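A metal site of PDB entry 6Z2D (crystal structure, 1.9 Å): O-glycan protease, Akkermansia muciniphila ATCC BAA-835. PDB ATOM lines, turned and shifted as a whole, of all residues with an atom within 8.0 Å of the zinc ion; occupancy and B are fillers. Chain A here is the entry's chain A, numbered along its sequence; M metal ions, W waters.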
ATOM      1  N   TYR A 143      32.475  24.265  17.094  1.00  0.00           N
ATOM      2  CA  TYR A 143      31.280  23.637  16.497  1.00  0.00           C
ATOM      3  C   TYR A 143      30.216  23.471  17.583  1.00  0.00           C
ATOM      4  O   TYR A 143      30.472  23.596  18.734  1.00  0.00           O
ATOM      5  CB  TYR A 143      31.593  22.227  15.989  1.00  0.00           C
ATOM      6  CG  TYR A 143      32.714  21.454  16.660  1.00  0.00           C
ATOM      7  CD1 TYR A 143      32.587  20.940  17.929  1.00  0.00           C
ATOM      8  CD2 TYR A 143      33.945  21.330  16.055  1.00  0.00           C
ATOM      9  CE1 TYR A 143      33.633  20.288  18.541  1.00  0.00           C
ATOM     10  CE2 TYR A 143      34.995  20.675  16.655  1.00  0.00           C
ATOM     11  CZ  TYR A 143      34.842  20.158  17.909  1.00  0.00           C
ATOM     12  OH  TYR A 143      35.851  19.499  18.521  1.00  0.00           O
ATOM     13  N   GLY A 144      28.992  23.219  17.135  1.00  0.00           N
ATOM     14  CA  GLY A 144      27.965  22.779  18.057  1.00  0.00           C
ATOM     15  C   GLY A 144      28.097  21.297  18.346  1.00  0.00           C
ATOM     16  O   GLY A 144      28.473  20.506  17.491  1.00  0.00           O
ATOM     17  N   GLY A 178      31.176  33.663  13.909  1.00  0.00           N
ATOM     18  CA  GLY A 178      31.284  32.231  14.133  1.00  0.00           C
ATOM     19  C   GLY A 178      30.715  31.805  15.467  1.00  0.00           C
ATOM     20  O   GLY A 178      29.954  30.834  15.553  1.00  0.00           O
ATOM     21  N   HIS A 181      26.933  31.931  15.476  1.00  0.00           N
ATOM     22  CA  HIS A 181      26.328  30.839  14.714  1.00  0.00           C
ATOM     23  C   HIS A 181      26.446  29.528  15.478  1.00  0.00           C
ATOM     24  O   HIS A 181      25.481  28.755  15.540  1.00  0.00           O
ATOM     25  CB  HIS A 181      27.019  30.764  13.349  1.00  0.00           C
ATOM     26  CG  HIS A 181      26.600  29.599  12.492  1.00  0.00           C
ATOM     27  ND1 HIS A 181      25.862  29.762  11.339  1.00  0.00           N
ATOM     28  CD2 HIS A 181      26.886  28.277  12.580  1.00  0.00           C
ATOM     29  CE1 HIS A 181      25.667  28.581  10.774  1.00  0.00           C
ATOM     30  NE2 HIS A 181      26.289  27.665  11.492  1.00  0.00           N
ATOM     31  N   GLU A 182      27.622  29.244  16.051  1.00  0.00           N
ATOM     32  CA  GLU A 182      27.777  28.008  16.815  1.00  0.00           C
ATOM     33  C   GLU A 182      26.906  28.031  18.059  1.00  0.00           C
ATOM     34  O   GLU A 182      26.366  26.993  18.457  1.00  0.00           O
ATOM     35  CB  GLU A 182      29.238  27.791  17.225  1.00  0.00           C
ATOM     36  CG  GLU A 182      30.226  27.783  16.078  1.00  0.00           C
ATOM     37  CD  GLU A 182      29.990  26.684  15.037  1.00  0.00           C
ATOM     38  OE1 GLU A 182      29.283  25.703  15.322  1.00  0.00           O
ATOM     39  OE2 GLU A 182      30.544  26.825  13.928  1.00  0.00           O
ATOM     40  N   GLY A 184      24.053  29.405  18.187  1.00  0.00           N
ATOM     41  CA  GLY A 184      22.729  29.054  17.698  1.00  0.00           C
ATOM     42  C   GLY A 184      22.524  27.556  17.655  1.00  0.00           C
ATOM     43  O   GLY A 184      21.507  27.042  18.122  1.00  0.00           O
ATOM     44  N   HIS A 185      23.508  26.820  17.108  1.00  0.00           N
ATOM     45  CA  HIS A 185      23.468  25.361  17.132  1.00  0.00           C
ATOM     46  C   HIS A 185      23.329  24.843  18.556  1.00  0.00           C
ATOM     47  O   HIS A 185      22.504  23.956  18.822  1.00  0.00           O
ATOM     48  CB  HIS A 185      24.735  24.788  16.497  1.00  0.00           C
ATOM     49  CG  HIS A 185      24.784  24.903  15.010  1.00  0.00           C
ATOM     50  ND1 HIS A 185      23.684  24.689  14.202  1.00  0.00           N
ATOM     51  CD2 HIS A 185      25.811  25.208  14.167  1.00  0.00           C
ATOM     52  CE1 HIS A 185      24.026  24.861  12.943  1.00  0.00           C
ATOM     53  NE2 HIS A 185      25.313  25.168  12.882  1.00  0.00           N
ATOM     54  N   LEU A 189      19.424  25.251  17.178  1.00  0.00           N
ATOM     55  CA  LEU A 189      19.039  25.770  15.862  1.00  0.00           C
ATOM     56  C   LEU A 189      19.727  24.982  14.740  1.00  0.00           C
ATOM     57  O   LEU A 189      20.948  24.796  14.789  1.00  0.00           O
ATOM     58  CB  LEU A 189      19.396  27.254  15.741  1.00  0.00           C
ATOM     59  CG  LEU A 189      18.746  28.237  16.735  1.00  0.00           C
ATOM     60  CD1 LEU A 189      18.989  29.691  16.302  1.00  0.00           C
ATOM     61  CD2 LEU A 189      17.263  27.972  16.776  1.00  0.00           C
ATOM     62  N   PRO A 190      18.995  24.532  13.724  1.00  0.00           N
ATOM     63  CA  PRO A 190      19.620  24.004  12.505  1.00  0.00           C
ATOM     64  C   PRO A 190      19.957  25.162  11.575  1.00  0.00           C
ATOM     65  O   PRO A 190      19.633  26.313  11.842  1.00  0.00           O
ATOM     66  CB  PRO A 190      18.527  23.122  11.917  1.00  0.00           C
ATOM     67  CG  PRO A 190      17.269  23.891  12.258  1.00  0.00           C
ATOM     68  CD  PRO A 190      17.524  24.500  13.636  1.00  0.00           C
ATOM     69  N   HIS A 191      20.589  24.841  10.450  1.00  0.00           N
ATOM     70  CA  HIS A 191      20.802  25.842   9.403  1.00  0.00           C
ATOM     71  C   HIS A 191      19.497  26.216   8.725  1.00  0.00           C
ATOM     72  O   HIS A 191      18.559  25.393   8.642  1.00  0.00           O
ATOM     73  CB  HIS A 191      21.782  25.316   8.351  1.00  0.00           C
ATOM     74  CG  HIS A 191      23.162  25.077   8.881  1.00  0.00           C
ATOM     75  ND1 HIS A 191      23.894  23.947   8.572  1.00  0.00           N
ATOM     76  CD2 HIS A 191      23.934  25.815   9.708  1.00  0.00           C
ATOM     77  CE1 HIS A 191      25.063  24.006   9.187  1.00  0.00           C
ATOM     78  NE2 HIS A 191      25.110  25.131   9.882  1.00  0.00           N
ATOM     79  N   ASN A 192      19.417  27.450   8.210  1.00  0.00           N
ATOM     80  CA  ASN A 192      18.291  27.772   7.346  1.00  0.00           C
ATOM     81  C   ASN A 192      18.617  29.006   6.531  1.00  0.00           C
ATOM     82  O   ASN A 192      19.555  29.747   6.830  1.00  0.00           O
ATOM     83  CB  ASN A 192      16.961  27.956   8.113  1.00  0.00           C
ATOM     84  CG  ASN A 192      16.960  29.149   9.087  1.00  0.00           C
ATOM     85  OD1 ASN A 192      17.971  29.838   9.269  1.00  0.00           O
ATOM     86  ND2 ASN A 192      15.793  29.416   9.659  1.00  0.00           N
ATOM     87  N   LEU A 206      21.220  34.441  10.407  1.00  0.00           N
ATOM     88  CA  LEU A 206      22.393  34.051  11.180  1.00  0.00           C
ATOM     89  C   LEU A 206      22.723  32.583  10.977  1.00  0.00           C
ATOM     90  O   LEU A 206      23.896  32.212  10.832  1.00  0.00           O
ATOM     91  CB  LEU A 206      22.186  34.349  12.671  1.00  0.00           C
ATOM     92  CG  LEU A 206      23.287  33.807  13.574  1.00  0.00           C
ATOM     93  CD1 LEU A 206      24.636  34.463  13.248  1.00  0.00           C
ATOM     94  CD2 LEU A 206      22.923  33.990  15.050  1.00  0.00           C
ATOM     95  N   MET A 207      21.705  31.709  10.982  1.00  0.00           N
ATOM     96  CA  MET A 207      21.981  30.290  10.835  1.00  0.00           C
ATOM     97  C   MET A 207      22.123  29.849   9.376  1.00  0.00           C
ATOM     98  O   MET A 207      22.173  28.648   9.097  1.00  0.00           O
ATOM     99  CB  MET A 207      20.879  29.474  11.534  1.00  0.00           C
ATOM    100  CG  MET A 207      20.821  29.745  13.044  1.00  0.00           C
ATOM    101  SD  MET A 207      22.441  29.706  13.863  1.00  0.00           S
ATOM    102  CE  MET A 207      22.975  28.027  13.506  1.00  0.00           C
ATOM    103  N   GLY A 208      22.168  30.798   8.445  1.00  0.00           N
ATOM    104  CA  GLY A 208      22.525  30.486   7.075  1.00  0.00           C
ATOM    105  C   GLY A 208      23.968  30.856   6.838  1.00  0.00           C
ATOM    106  O   GLY A 208      24.886  30.146   7.256  1.00  0.00           O
ATOM    107  N   ASN A 211      27.101  33.962   9.761  1.00  0.00           N
ATOM    108  CA  ASN A 211      28.395  33.975  10.431  1.00  0.00           C
ATOM    109  C   ASN A 211      29.436  34.711   9.606  1.00  0.00           C
ATOM    110  O   ASN A 211      30.495  35.059  10.151  1.00  0.00           O
ATOM    111  CB  ASN A 211      28.869  32.548  10.742  1.00  0.00           C
ATOM    112  CG  ASN A 211      28.802  31.620   9.533  1.00  0.00           C
ATOM    113  OD1 ASN A 211      28.126  31.887   8.545  1.00  0.00           O
ATOM    114  ND2 ASN A 211      29.528  30.507   9.626  1.00  0.00           N
ATOM    115  N   VAL A 290      23.391  17.420   7.335  1.00  0.00           N
ATOM    116  CA  VAL A 290      23.253  18.520   8.294  1.00  0.00           C
ATOM    117  C   VAL A 290      24.212  19.677   8.044  1.00  0.00           C
ATOM    118  O   VAL A 290      24.112  20.705   8.737  1.00  0.00           O
ATOM    119  CB  VAL A 290      23.431  18.013   9.737  1.00  0.00           C
ATOM    120  N   ASN A 291      25.157  19.545   7.104  1.00  0.00           N
ATOM    121  CA  ASN A 291      25.981  20.677   6.695  1.00  0.00           C
ATOM    122  C   ASN A 291      25.925  20.873   5.181  1.00  0.00           C
ATOM    123  O   ASN A 291      26.852  21.415   4.576  1.00  0.00           O
ATOM    124  CB  ASN A 291      27.424  20.530   7.166  1.00  0.00           C
ATOM    125  CG  ASN A 291      27.678  21.301   8.452  1.00  0.00           C
ATOM    126  OD1 ASN A 291      28.432  22.278   8.469  1.00  0.00           O
ATOM    127  ND2 ASN A 291      27.024  20.874   9.528  1.00  0.00           N
ATOM    128  N   ASP A 293      22.704  21.928   4.191  1.00  0.00           N
ATOM    129  CA  ASP A 293      21.368  22.486   4.350  1.00  0.00           C
ATOM    130  C   ASP A 293      21.394  23.982   4.683  1.00  0.00           C
ATOM    131  O   ASP A 293      20.391  24.506   5.170  1.00  0.00           O
ATOM    132  CB  ASP A 293      20.598  21.731   5.429  1.00  0.00           C
ATOM    133  CG  ASP A 293      21.332  21.720   6.762  1.00  0.00           C
ATOM    134  OD1 ASP A 293      22.516  22.133   6.812  1.00  0.00           O
ATOM    135  OD2 ASP A 293      20.729  21.273   7.760  1.00  0.00           O
ATOM    136  N   TYR A 294      22.521  24.677   4.443  1.00  0.00           N
ATOM    137  CA  TYR A 294      22.504  26.132   4.526  1.00  0.00           C
ATOM    138  C   TYR A 294      21.478  26.729   3.592  1.00  0.00           C
ATOM    139  O   TYR A 294      21.074  27.887   3.767  1.00  0.00           O
ATOM    140  CB  TYR A 294      23.881  26.711   4.189  1.00  0.00           C
ATOM    141  CG  TYR A 294      24.993  26.186   5.061  1.00  0.00           C
ATOM    142  CD1 TYR A 294      25.278  26.782   6.292  1.00  0.00           C
ATOM    143  CD2 TYR A 294      25.761  25.093   4.662  1.00  0.00           C
ATOM    144  CE1 TYR A 294      26.299  26.300   7.098  1.00  0.00           C
ATOM    145  CE2 TYR A 294      26.779  24.599   5.455  1.00  0.00           C
ATOM    146  CZ  TYR A 294      27.051  25.207   6.673  1.00  0.00           C
ATOM    147  OH  TYR A 294      28.066  24.730   7.460  1.00  0.00           O
HETATM  148 ZN    ZN M   1      26.521  25.639  11.271  1.00  0.00          ZN
HETATM  149  O   HOH W   1      27.514  23.423  11.197  1.00  0.00           O
HETATM  150  O   HOH W   2      28.601  25.492  12.254  1.00  0.00           O
HETATM  151  O   HOH W   3      28.266  25.624   9.802  1.00  0.00           O
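ND1 of His 191 lies within hydrogen-bond range of O of Val 290. The backbone carbonyl oxygen (O) of Leu 206 sits at hydrogen-bond distance from a ring nitrogen (ND1) of His 181, at 3.2 Å. The side-chain carboxylate (OD1) of Asp 293 sits at hydrogen-bond distance from a ring nitrogen (ND1) of His 191. A ring nitrogen (ND1) of His 185 sits at hydrogen-bond distance from the backbone carbonyl oxygen (O) of Leu 189, 2.8 Å away.
The zinc ion is bound by NE2 of His 191, NE2 of His 181, NE2 of His 185, water W3, water W2 and water W1.
Three residues have an atom within 4 Å of the zinc ion: His 181, His 185 and His 191. The nearest printed residue that does not touch the zinc ion is Tyr 294 (4.2 Å).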
